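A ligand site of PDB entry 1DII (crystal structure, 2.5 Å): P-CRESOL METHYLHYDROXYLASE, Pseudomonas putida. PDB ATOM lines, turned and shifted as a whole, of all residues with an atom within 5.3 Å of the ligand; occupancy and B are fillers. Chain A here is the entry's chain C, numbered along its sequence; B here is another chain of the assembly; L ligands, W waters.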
ATOM      1  N   LEU A  10      15.308  22.258   5.328  1.00  0.00           N
ATOM      2  CA  LEU A  10      16.748  22.208   5.054  1.00  0.00           C
ATOM      3  C   LEU A  10      17.479  21.650   6.272  1.00  0.00           C
ATOM      4  O   LEU A  10      18.414  20.865   6.134  1.00  0.00           O
ATOM      5  CB  LEU A  10      17.300  23.597   4.735  1.00  0.00           C
ATOM      6  CG  LEU A  10      18.825  23.784   4.561  1.00  0.00           C
ATOM      7  CD1 LEU A  10      19.406  22.865   3.501  1.00  0.00           C
ATOM      8  CD2 LEU A  10      19.098  25.209   4.165  1.00  0.00           C
ATOM      9  N   VAL A  14      19.351  18.152   5.662  1.00  0.00           N
ATOM     10  CA  VAL A  14      20.806  18.285   5.554  1.00  0.00           C
ATOM     11  C   VAL A  14      21.537  18.501   6.872  1.00  0.00           C
ATOM     12  O   VAL A  14      22.115  17.568   7.429  1.00  0.00           O
ATOM     13  CB  VAL A  14      21.210  19.390   4.530  1.00  0.00           C
ATOM     14  CG1 VAL A  14      22.734  19.485   4.371  1.00  0.00           C
ATOM     15  CG2 VAL A  14      20.588  19.122   3.213  1.00  0.00           C
ATOM     16  N   CYS A  15      21.466  19.733   7.394  1.00  0.00           N
ATOM     17  CA  CYS A  15      22.146  20.156   8.612  1.00  0.00           C
ATOM     18  C   CYS A  15      21.946  19.323   9.881  1.00  0.00           C
ATOM     19  O   CYS A  15      22.920  18.909  10.493  1.00  0.00           O
ATOM     20  CB  CYS A  15      21.826  21.617   8.889  1.00  0.00           C
ATOM     21  SG  CYS A  15      21.656  22.691   7.440  1.00  0.00           S
ATOM     22  N   CYS A  18      23.971  16.098  11.229  1.00  0.00           N
ATOM     23  CA  CYS A  18      25.240  16.263  11.926  1.00  0.00           C
ATOM     24  C   CYS A  18      25.059  17.130  13.179  1.00  0.00           C
ATOM     25  O   CYS A  18      25.637  16.853  14.231  1.00  0.00           O
ATOM     26  CB  CYS A  18      26.246  16.931  11.014  1.00  0.00           C
ATOM     27  SG  CYS A  18      26.898  15.890   9.693  1.00  0.00           S
ATOM     28  N   HIS A  19      24.221  18.145  13.051  1.00  0.00           N
ATOM     29  CA  HIS A  19      23.953  19.131  14.085  1.00  0.00           C
ATOM     30  C   HIS A  19      22.928  18.906  15.170  1.00  0.00           C
ATOM     31  O   HIS A  19      23.076  19.493  16.226  1.00  0.00           O
ATOM     32  CB  HIS A  19      23.772  20.488  13.442  1.00  0.00           C
ATOM     33  CG  HIS A  19      25.074  21.093  12.987  1.00  0.00           C
ATOM     34  ND1 HIS A  19      25.981  21.535  13.898  1.00  0.00           N
ATOM     35  CD2 HIS A  19      25.332  21.198  11.676  1.00  0.00           C
ATOM     36  CE1 HIS A  19      26.969  21.976  13.043  1.00  0.00           C
ATOM     37  NE2 HIS A  19      26.585  21.775  11.700  1.00  0.00           N
ATOM     38  N   VAL A  25      27.805  15.396  15.693  1.00  0.00           N
ATOM     39  CA  VAL A  25      29.023  15.476  14.862  1.00  0.00           C
ATOM     40  C   VAL A  25      29.462  16.940  14.871  1.00  0.00           C
ATOM     41  O   VAL A  25      30.650  17.252  14.894  1.00  0.00           O
ATOM     42  CB  VAL A  25      28.766  14.998  13.404  1.00  0.00           C
ATOM     43  CG1 VAL A  25      29.993  15.271  12.481  1.00  0.00           C
ATOM     44  CG2 VAL A  25      28.427  13.536  13.403  1.00  0.00           C
ATOM     45  N   GLY A  26      28.463  17.813  14.860  1.00  0.00           N
ATOM     46  CA  GLY A  26      28.713  19.238  14.912  1.00  0.00           C
ATOM     47  C   GLY A  26      28.059  19.847  16.144  1.00  0.00           C
ATOM     48  O   GLY A  26      27.188  19.212  16.745  1.00  0.00           O
ATOM     49  N   PRO A  27      28.460  21.064  16.563  1.00  0.00           N
ATOM     50  CA  PRO A  27      27.856  21.705  17.755  1.00  0.00           C
ATOM     51  C   PRO A  27      26.391  22.078  17.555  1.00  0.00           C
ATOM     52  O   PRO A  27      25.916  22.152  16.417  1.00  0.00           O
ATOM     53  CB  PRO A  27      28.733  22.953  17.929  1.00  0.00           C
ATOM     54  CG  PRO A  27      29.210  23.264  16.540  1.00  0.00           C
ATOM     55  CD  PRO A  27      29.557  21.889  16.033  1.00  0.00           C
ATOM     56  N   VAL A  28      25.674  22.277  18.650  1.00  0.00           N
ATOM     57  CA  VAL A  28      24.259  22.661  18.609  1.00  0.00           C
ATOM     58  C   VAL A  28      24.125  24.068  18.033  1.00  0.00           C
ATOM     59  O   VAL A  28      24.934  24.942  18.312  1.00  0.00           O
ATOM     60  CB  VAL A  28      23.615  22.568  20.015  1.00  0.00           C
ATOM     61  CG1 VAL A  28      22.140  22.927  19.965  1.00  0.00           C
ATOM     62  CG2 VAL A  28      23.780  21.140  20.569  1.00  0.00           C
ATOM     63  N   LEU A  29      23.176  24.239  17.127  1.00  0.00           N
ATOM     64  CA  LEU A  29      22.930  25.526  16.494  1.00  0.00           C
ATOM     65  C   LEU A  29      21.570  26.088  16.930  1.00  0.00           C
ATOM     66  O   LEU A  29      21.307  27.299  16.762  1.00  0.00           O
ATOM     67  CB  LEU A  29      22.954  25.377  14.975  1.00  0.00           C
ATOM     68  CG  LEU A  29      24.176  24.843  14.215  1.00  0.00           C
ATOM     69  CD1 LEU A  29      23.827  24.733  12.730  1.00  0.00           C
ATOM     70  CD2 LEU A  29      25.378  25.741  14.423  1.00  0.00           C
ATOM     71  N   ARG A  32      20.849  29.506  19.545  1.00  0.00           N
ATOM     72  CA  ARG A  32      22.110  30.092  19.971  1.00  0.00           C
ATOM     73  C   ARG A  32      22.268  31.526  19.456  1.00  0.00           C
ATOM     74  O   ARG A  32      23.182  32.246  19.865  1.00  0.00           O
ATOM     75  CB  ARG A  32      23.273  29.192  19.567  1.00  0.00           C
ATOM     76  CG  ARG A  32      23.648  28.169  20.638  1.00  0.00           C
ATOM     77  CD  ARG A  32      24.939  27.427  20.319  1.00  0.00           C
ATOM     78  NE  ARG A  32      26.015  28.317  19.857  1.00  0.00           N
ATOM     79  CZ  ARG A  32      26.958  27.968  18.976  1.00  0.00           C
ATOM     80  NH1 ARG A  32      26.993  26.754  18.440  1.00  0.00           N
ATOM     81  NH2 ARG A  32      27.882  28.861  18.623  1.00  0.00           N
ATOM     82  N   LEU A  34      22.968  32.679  16.360  1.00  0.00           N
ATOM     83  CA  LEU A  34      24.060  32.941  15.424  1.00  0.00           C
ATOM     84  C   LEU A  34      23.570  33.764  14.227  1.00  0.00           C
ATOM     85  O   LEU A  34      22.535  33.459  13.651  1.00  0.00           O
ATOM     86  CB  LEU A  34      24.693  31.646  14.912  1.00  0.00           C
ATOM     87  CG  LEU A  34      25.327  30.613  15.849  1.00  0.00           C
ATOM     88  CD1 LEU A  34      24.338  29.496  16.067  1.00  0.00           C
ATOM     89  CD2 LEU A  34      26.538  30.033  15.182  1.00  0.00           C
ATOM     90  N   TYR A  38      27.028  34.830   9.354  1.00  0.00           N
ATOM     91  CA  TYR A  38      28.010  33.867   9.833  1.00  0.00           C
ATOM     92  C   TYR A  38      27.680  32.477   9.278  1.00  0.00           C
ATOM     93  O   TYR A  38      28.572  31.788   8.765  1.00  0.00           O
ATOM     94  CB  TYR A  38      28.076  33.837  11.367  1.00  0.00           C
ATOM     95  CG  TYR A  38      29.075  32.815  11.918  1.00  0.00           C
ATOM     96  CD1 TYR A  38      30.464  32.902  11.608  1.00  0.00           C
ATOM     97  CD2 TYR A  38      28.617  31.753  12.716  1.00  0.00           C
ATOM     98  CE1 TYR A  38      31.378  31.938  12.107  1.00  0.00           C
ATOM     99  CE2 TYR A  38      29.507  30.774  13.214  1.00  0.00           C
ATOM    100  CZ  TYR A  38      30.880  30.872  12.915  1.00  0.00           C
ATOM    101  OH  TYR A  38      31.710  29.893  13.440  1.00  0.00           O
ATOM    102  N   ILE A  39      26.411  32.092   9.404  1.00  0.00           N
ATOM    103  CA  ILE A  39      25.890  30.823   8.888  1.00  0.00           C
ATOM    104  C   ILE A  39      26.123  30.689   7.369  1.00  0.00           C
ATOM    105  O   ILE A  39      26.369  29.587   6.885  1.00  0.00           O
ATOM    106  CB  ILE A  39      24.390  30.653   9.268  1.00  0.00           C
ATOM    107  CG1 ILE A  39      24.275  30.447  10.783  1.00  0.00           C
ATOM    108  CG2 ILE A  39      23.757  29.479   8.522  1.00  0.00           C
ATOM    109  CD1 ILE A  39      22.889  30.096  11.322  1.00  0.00           C
ATOM    110  N   ILE A  42      30.134  30.053   6.819  1.00  0.00           N
ATOM    111  CA  ILE A  42      30.524  28.697   7.218  1.00  0.00           C
ATOM    112  C   ILE A  42      30.047  27.708   6.152  1.00  0.00           C
ATOM    113  O   ILE A  42      30.810  26.841   5.739  1.00  0.00           O
ATOM    114  CB  ILE A  42      29.971  28.295   8.621  1.00  0.00           C
ATOM    115  CG1 ILE A  42      30.650  29.124   9.718  1.00  0.00           C
ATOM    116  CG2 ILE A  42      30.245  26.828   8.923  1.00  0.00           C
ATOM    117  CD1 ILE A  42      32.198  29.129   9.703  1.00  0.00           C
ATOM    118  N   VAL A  43      28.817  27.878   5.664  1.00  0.00           N
ATOM    119  CA  VAL A  43      28.287  26.980   4.632  1.00  0.00           C
ATOM    120  C   VAL A  43      29.001  27.140   3.280  1.00  0.00           C
ATOM    121  O   VAL A  43      29.322  26.149   2.627  1.00  0.00           O
ATOM    122  CB  VAL A  43      26.754  27.111   4.511  1.00  0.00           C
ATOM    123  CG1 VAL A  43      26.210  26.257   3.381  1.00  0.00           C
ATOM    124  CG2 VAL A  43      26.121  26.623   5.776  1.00  0.00           C
ATOM    125  N   PHE A  47      34.123  24.674   7.238  1.00  0.00           N
ATOM    126  CA  PHE A  47      34.967  24.997   8.367  1.00  0.00           C
ATOM    127  C   PHE A  47      35.597  23.746   8.945  1.00  0.00           C
ATOM    128  O   PHE A  47      34.956  22.986   9.693  1.00  0.00           O
ATOM    129  CB  PHE A  47      34.174  25.775   9.425  1.00  0.00           C
ATOM    130  CG  PHE A  47      35.019  26.248  10.590  1.00  0.00           C
ATOM    131  CD1 PHE A  47      36.173  27.029  10.380  1.00  0.00           C
ATOM    132  CD2 PHE A  47      34.666  25.871  11.902  1.00  0.00           C
ATOM    133  CE1 PHE A  47      36.985  27.432  11.458  1.00  0.00           C
ATOM    134  CE2 PHE A  47      35.468  26.246  13.011  1.00  0.00           C
ATOM    135  CZ  PHE A  47      36.639  27.043  12.781  1.00  0.00           C
ATOM    136  N   ARG A  48      36.872  23.554   8.614  1.00  0.00           N
ATOM    137  CA  ARG A  48      37.658  22.413   9.089  1.00  0.00           C
ATOM    138  C   ARG A  48      36.961  21.051   8.828  1.00  0.00           C
ATOM    139  O   ARG A  48      36.925  20.600   7.686  1.00  0.00           O
ATOM    140  CB  ARG A  48      38.066  22.616  10.562  1.00  0.00           C
ATOM    141  CG  ARG A  48      38.819  23.945  10.810  1.00  0.00           C
ATOM    142  CD  ARG A  48      39.476  24.049  12.173  1.00  0.00           C
ATOM    143  NE  ARG A  48      38.562  23.807  13.273  1.00  0.00           N
ATOM    144  CZ  ARG A  48      38.582  24.449  14.441  1.00  0.00           C
ATOM    145  NH1 ARG A  48      39.492  25.405  14.673  1.00  0.00           N
ATOM    146  NH2 ARG A  48      37.698  24.124  15.388  1.00  0.00           N
ATOM    147  N   ALA A  49      36.396  20.418   9.856  1.00  0.00           N
ATOM    148  CA  ALA A  49      35.709  19.121   9.690  1.00  0.00           C
ATOM    149  C   ALA A  49      34.414  19.232   8.879  1.00  0.00           C
ATOM    150  O   ALA A  49      34.003  18.280   8.211  1.00  0.00           O
ATOM    151  CB  ALA A  49      35.412  18.497  11.040  1.00  0.00           C
ATOM    152  N   MET A  50      33.792  20.402   8.923  1.00  0.00           N
ATOM    153  CA  MET A  50      32.555  20.673   8.204  1.00  0.00           C
ATOM    154  C   MET A  50      32.768  20.947   6.719  1.00  0.00           C
ATOM    155  O   MET A  50      33.625  21.748   6.357  1.00  0.00           O
ATOM    156  CB  MET A  50      31.811  21.898   8.783  1.00  0.00           C
ATOM    157  CG  MET A  50      30.447  22.075   8.096  1.00  0.00           C
ATOM    158  SD  MET A  50      29.282  23.196   8.671  1.00  0.00           S
ATOM    159  CE  MET A  50      28.637  23.655   7.144  1.00  0.00           C
ATOM    160  N   PRO A  51      31.979  20.264   5.842  1.00  0.00           N
ATOM    161  CA  PRO A  51      32.126  20.503   4.412  1.00  0.00           C
ATOM    162  C   PRO A  51      31.425  21.786   3.942  1.00  0.00           C
ATOM    163  O   PRO A  51      30.687  22.421   4.692  1.00  0.00           O
ATOM    164  CB  PRO A  51      31.481  19.267   3.805  1.00  0.00           C
ATOM    165  CG  PRO A  51      30.508  18.796   4.834  1.00  0.00           C
ATOM    166  CD  PRO A  51      31.227  19.010   6.093  1.00  0.00           C
ATOM    167  N   PHE A  53      28.946  23.666   1.076  1.00  0.00           N
ATOM    168  CA  PHE A  53      27.839  23.390   0.156  1.00  0.00           C
ATOM    169  C   PHE A  53      27.757  24.532  -0.868  1.00  0.00           C
ATOM    170  O   PHE A  53      27.735  25.715  -0.486  1.00  0.00           O
ATOM    171  CB  PHE A  53      26.508  23.258   0.911  1.00  0.00           C
ATOM    172  CG  PHE A  53      26.447  22.075   1.843  1.00  0.00           C
ATOM    173  CD1 PHE A  53      26.947  22.154   3.147  1.00  0.00           C
ATOM    174  CD2 PHE A  53      25.923  20.857   1.397  1.00  0.00           C
ATOM    175  CE1 PHE A  53      26.929  21.027   4.023  1.00  0.00           C
ATOM    176  CE2 PHE A  53      25.887  19.721   2.265  1.00  0.00           C
ATOM    177  CZ  PHE A  53      26.399  19.818   3.580  1.00  0.00           C
ATOM    178  N   VAL A  58      22.605  24.294  -1.758  1.00  0.00           N
ATOM    179  CA  VAL A  58      21.870  25.095  -0.772  1.00  0.00           C
ATOM    180  C   VAL A  58      22.027  26.569  -1.175  1.00  0.00           C
ATOM    181  O   VAL A  58      23.086  27.161  -0.927  1.00  0.00           O
ATOM    182  CB  VAL A  58      22.448  24.929   0.700  1.00  0.00           C
ATOM    183  CG1 VAL A  58      21.636  25.706   1.679  1.00  0.00           C
ATOM    184  CG2 VAL A  58      22.487  23.471   1.155  1.00  0.00           C
ATOM    185  N   LEU A  63      19.397  29.630   3.029  1.00  0.00           N
ATOM    186  CA  LEU A  63      20.344  29.928   4.100  1.00  0.00           C
ATOM    187  C   LEU A  63      19.749  30.927   5.107  1.00  0.00           C
ATOM    188  O   LEU A  63      19.869  30.743   6.322  1.00  0.00           O
ATOM    189  CB  LEU A  63      21.653  30.418   3.506  1.00  0.00           C
ATOM    190  CG  LEU A  63      22.929  29.610   3.786  1.00  0.00           C
ATOM    191  CD1 LEU A  63      22.652  28.150   4.210  1.00  0.00           C
ATOM    192  CD2 LEU A  63      23.810  29.720   2.561  1.00  0.00           C
ATOM    193  N   VAL A  66      16.979  29.009   7.110  1.00  0.00           N
ATOM    194  CA  VAL A  66      17.541  28.142   8.159  1.00  0.00           C
ATOM    195  C   VAL A  66      18.099  28.956   9.329  1.00  0.00           C
ATOM    196  O   VAL A  66      17.925  28.566  10.498  1.00  0.00           O
ATOM    197  CB  VAL A  66      18.581  27.084   7.595  1.00  0.00           C
ATOM    198  CG1 VAL A  66      19.932  27.716   7.281  1.00  0.00           C
ATOM    199  CG2 VAL A  66      18.695  25.865   8.533  1.00  0.00           C
ATOM    200  N   LEU A  70      16.625  28.609  13.182  1.00  0.00           N
ATOM    201  CA  LEU A  70      17.546  28.281  14.257  1.00  0.00           C
ATOM    202  C   LEU A  70      17.442  29.218  15.448  1.00  0.00           C
ATOM    203  O   LEU A  70      17.465  28.746  16.588  1.00  0.00           O
ATOM    204  CB  LEU A  70      18.987  28.232  13.734  1.00  0.00           C
ATOM    205  CG  LEU A  70      19.671  26.909  13.349  1.00  0.00           C
ATOM    206  CD1 LEU A  70      18.775  25.664  13.412  1.00  0.00           C
ATOM    207  CD2 LEU A  70      20.315  27.087  11.987  1.00  0.00           C
ATOM    208  N   ILE B 158      23.326  13.128   1.993  1.00  0.00           N
ATOM    209  CA  ILE B 158      23.829  14.214   1.175  1.00  0.00           C
ATOM    210  C   ILE B 158      24.535  13.817  -0.113  1.00  0.00           C
ATOM    211  O   ILE B 158      24.799  14.675  -0.951  1.00  0.00           O
ATOM    212  CB  ILE B 158      24.736  15.204   1.992  1.00  0.00           C
ATOM    213  CG1 ILE B 158      25.992  14.517   2.528  1.00  0.00           C
ATOM    214  CG2 ILE B 158      23.910  15.871   3.100  1.00  0.00           C
ATOM    215  CD1 ILE B 158      27.112  15.480   2.956  1.00  0.00           C
ATOM    216  N   LEU B 378      24.483  10.457   9.300  1.00  0.00           N
ATOM    217  CA  LEU B 378      25.864  10.903   9.055  1.00  0.00           C
ATOM    218  C   LEU B 378      26.785  10.757  10.269  1.00  0.00           C
ATOM    219  O   LEU B 378      27.837  11.414  10.366  1.00  0.00           O
ATOM    220  CB  LEU B 378      25.898  12.359   8.520  1.00  0.00           C
ATOM    221  CG  LEU B 378      25.283  12.818   7.187  1.00  0.00           C
ATOM    222  CD1 LEU B 378      26.262  13.721   6.423  1.00  0.00           C
ATOM    223  CD2 LEU B 378      24.900  11.673   6.317  1.00  0.00           C
ATOM    224  N   PHE B 381      30.721  10.566  10.424  1.00  0.00           N
ATOM    225  CA  PHE B 381      31.475  11.779  10.155  1.00  0.00           C
ATOM    226  C   PHE B 381      32.257  12.237  11.395  1.00  0.00           C
ATOM    227  O   PHE B 381      33.098  13.149  11.330  1.00  0.00           O
ATOM    228  CB  PHE B 381      30.562  12.885   9.639  1.00  0.00           C
ATOM    229  CG  PHE B 381      30.437  12.886   8.153  1.00  0.00           C
ATOM    230  CD1 PHE B 381      31.104  13.854   7.388  1.00  0.00           C
ATOM    231  CD2 PHE B 381      29.701  11.886   7.502  1.00  0.00           C
ATOM    232  CE1 PHE B 381      31.035  13.854   5.948  1.00  0.00           C
ATOM    233  CE2 PHE B 381      29.610  11.854   6.078  1.00  0.00           C
ATOM    234  CZ  PHE B 381      30.277  12.850   5.305  1.00  0.00           C
ATOM    235  N   ASN B 385      36.361  14.197  13.593  1.00  0.00           N
ATOM    236  CA  ASN B 385      36.462  14.886  14.867  1.00  0.00           C
ATOM    237  C   ASN B 385      37.497  14.241  15.769  1.00  0.00           C
ATOM    238  O   ASN B 385      37.850  14.826  16.792  1.00  0.00           O
ATOM    239  CB  ASN B 385      35.100  14.926  15.556  1.00  0.00           C
ATOM    240  CG  ASN B 385      34.121  15.806  14.824  1.00  0.00           C
ATOM    241  OD1 ASN B 385      34.497  16.770  14.169  1.00  0.00           O
ATOM    242  ND2 ASN B 385      32.828  15.473  14.928  1.00  0.00           N
ATOM    243  N   GLY B 389      40.416  19.465  12.382  1.00  0.00           N
ATOM    244  CA  GLY B 389      41.231  20.174  11.409  1.00  0.00           C
ATOM    245  C   GLY B 389      40.872  19.998   9.953  1.00  0.00           C
ATOM    246  O   GLY B 389      41.375  20.734   9.101  1.00  0.00           O
HETATM  247 FE1  LIG L   1      27.808  22.403  10.205  1.00  0.00          FE
HETATM  248  C1  LIG L   1      30.069  23.654  12.414  1.00  0.00           C
HETATM  249  C2  LIG L   1      26.226  25.418  10.010  1.00  0.00           C
HETATM  250  C3  LIG L   1      25.589  21.126   7.885  1.00  0.00           C
HETATM  251  C4  LIG L   1      29.258  19.356  10.419  1.00  0.00           C
HETATM  252  N1  LIG L   1      28.084  24.213  11.055  1.00  0.00           N
HETATM  253  C5  LIG L   1      29.085  24.538  11.945  1.00  0.00           C
HETATM  254  C6  LIG L   1      28.924  25.954  12.315  1.00  0.00           C
HETATM  255  C7  LIG L   1      27.865  26.439  11.647  1.00  0.00           C
HETATM  256  C8  LIG L   1      27.311  25.358  10.843  1.00  0.00           C
HETATM  257  C9  LIG L   1      27.292  27.862  11.696  1.00  0.00           C
HETATM  258  C10 LIG L   1      29.834  26.684  13.303  1.00  0.00           C
HETATM  259  C11 LIG L   1      29.321  26.441  14.719  1.00  0.00           C
HETATM  260  C12 LIG L   1      29.998  27.263  15.793  1.00  0.00           C
HETATM  261  O1  LIG L   1      29.552  27.083  16.978  1.00  0.00           O
HETATM  262  O2  LIG L   1      30.909  28.029  15.461  1.00  0.00           O
HETATM  263  N2  LIG L   1      26.217  23.116   9.164  1.00  0.00           N
HETATM  264  C13 LIG L   1      25.723  24.412   9.234  1.00  0.00           C
HETATM  265  C14 LIG L   1      24.563  24.539   8.379  1.00  0.00           C
HETATM  266  C15 LIG L   1      24.388  23.332   7.768  1.00  0.00           C
HETATM  267  C16 LIG L   1      25.407  22.457   8.243  1.00  0.00           C
HETATM  268  C17 LIG L   1      23.734  25.818   8.219  1.00  0.00           C
HETATM  269  C18 LIG L   1      23.308  22.894   6.748  1.00  0.00           C
HETATM  270  C19 LIG L   1      23.325  23.715   5.441  1.00  0.00           C
HETATM  271  N3  LIG L   1      27.514  20.610   9.339  1.00  0.00           N
HETATM  272  C20 LIG L   1      26.543  20.270   8.399  1.00  0.00           C
HETATM  273  C21 LIG L   1      26.642  18.858   8.043  1.00  0.00           C
HETATM  274  C22 LIG L   1      27.654  18.371   8.780  1.00  0.00           C
HETATM  275  C23 LIG L   1      28.196  19.448   9.570  1.00  0.00           C
HETATM  276  C24 LIG L   1      25.717  18.127   7.027  1.00  0.00           C
HETATM  277  C25 LIG L   1      28.178  16.933   8.878  1.00  0.00           C
HETATM  278  C26 LIG L   1      28.781  16.341   7.603  1.00  0.00           C
HETATM  279  N4  LIG L   1      29.342  21.654  11.199  1.00  0.00           N
HETATM  280  C27 LIG L   1      29.823  20.348  11.172  1.00  0.00           C
HETATM  281  C28 LIG L   1      30.971  20.199  12.029  1.00  0.00           C
HETATM  282  C29 LIG L   1      31.210  21.405  12.584  1.00  0.00           C
HETATM  283  C30 LIG L   1      30.195  22.316  12.081  1.00  0.00           C
HETATM  284  C31 LIG L   1      31.776  18.887  12.250  1.00  0.00           C
HETATM  285  C32 LIG L   1      32.349  21.705  13.536  1.00  0.00           C
HETATM  286  C33 LIG L   1      33.562  22.140  12.661  1.00  0.00           C
HETATM  287  C34 LIG L   1      34.780  22.439  13.460  1.00  0.00           C
HETATM  288  O3  LIG L   1      34.721  23.240  14.417  1.00  0.00           O
HETATM  289  O4  LIG L   1      35.802  21.834  13.080  1.00  0.00           O
HETATM  290  O   HOH W   1      38.037  20.213  13.993  1.00  0.00           O
HETATM  291  O   HOH W   2      32.847  15.971  11.470  1.00  0.00           O
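An oxygen (O2) of the ligand is in hydrogen-bond range of the side-chain hydroxyl (OH) of Tyr 38 (2.9 Å). FE1 of the ligand is bound by NE2 of His 19. The side-chain sulfur (SG) of Cys 15 is covalently linked to a carbon (C18) of the ligand. The side-chain sulfur (SG) of Cys 18 is bonded to a carbon (C25) of the ligand (1.8 Å). The guanidinium group of Arg 32 is in salt-bridge range of an oxygen (O1) of the ligand, 2.9 Å away. The guanidinium group of Arg 48 is in salt-bridge range of an oxygen (O3) of the ligand (3.3 Å). FE1 of the ligand is bound by SD of Met 50 (2.3 Å).
Water W1 bridges an oxygen (O4) of the ligand and the backbone NH (N) of Gly 389 of chain B. Water W2 lies within hydrogen-bond range of the backbone carbonyl oxygen of Phe 381 of chain B (2.8 Å) and the side-chain amide oxygen of Asn 385 of chain B (3.3 Å).
Residues that only touch the ligand: Val 25, Phe 47, Phe 381 of chain B, Val 43, Ala 49, Ile 42, Pro 27, Val 14, Ile 39, Leu 29, Gly 26, Leu 378 of chain B, Phe 53, Pro 51 and Asn 385 of chain B. Hydrophobic or aromatic side chains that line the ligand: His 19, Pro 27, Leu 29, Tyr 38, Ile 39, Ile 42, Val 43, Phe 47, Ala 49, Met 50, Pro 51, Phe 53, Leu 378 of chain B and Phe 381 of chain B. Within 4 Å of the ligand: Val 14, Cys 15, Cys 18, His 19, Val 25, Gly 26, Pro 27, Leu 29, Arg 32, Tyr 38, Ile 39, Ile 42, Val 43, Phe 47, Arg 48, Ala 49, Met 50, Pro 51, Phe 53, Leu 378 of chain B, Phe 381 of chain B and Asn 385 of chain B. The nearest printed residue that does not touch the ligand is Leu 34 (4.2 Å).
The backbone carbonyl oxygen (O) of Val 43 is in hydrogen-bond range of the backbone NH (N) of Phe 53 (3.0 Å). The side-chain amide nitrogen of Asn 385 of chain B sits at hydrogen-bond distance from the backbone carbonyl oxygen of Val 25 (2.8 Å). O of Cys 18 sits at hydrogen-bond distance from N of Val 25, 3.0 Å away. O of Cys 18 is in hydrogen-bond range of N of Gly 26, at 3.1 Å. The guanidinium group (NH1) of Arg 32 sits at hydrogen-bond distance from the backbone carbonyl oxygen (O) of Val 28 (2.7 Å). N of Cys 15 is in hydrogen-bond range of O of Leu 10 (3.5 Å). ND1 of His 19 sits at hydrogen-bond distance from O of Pro 27.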
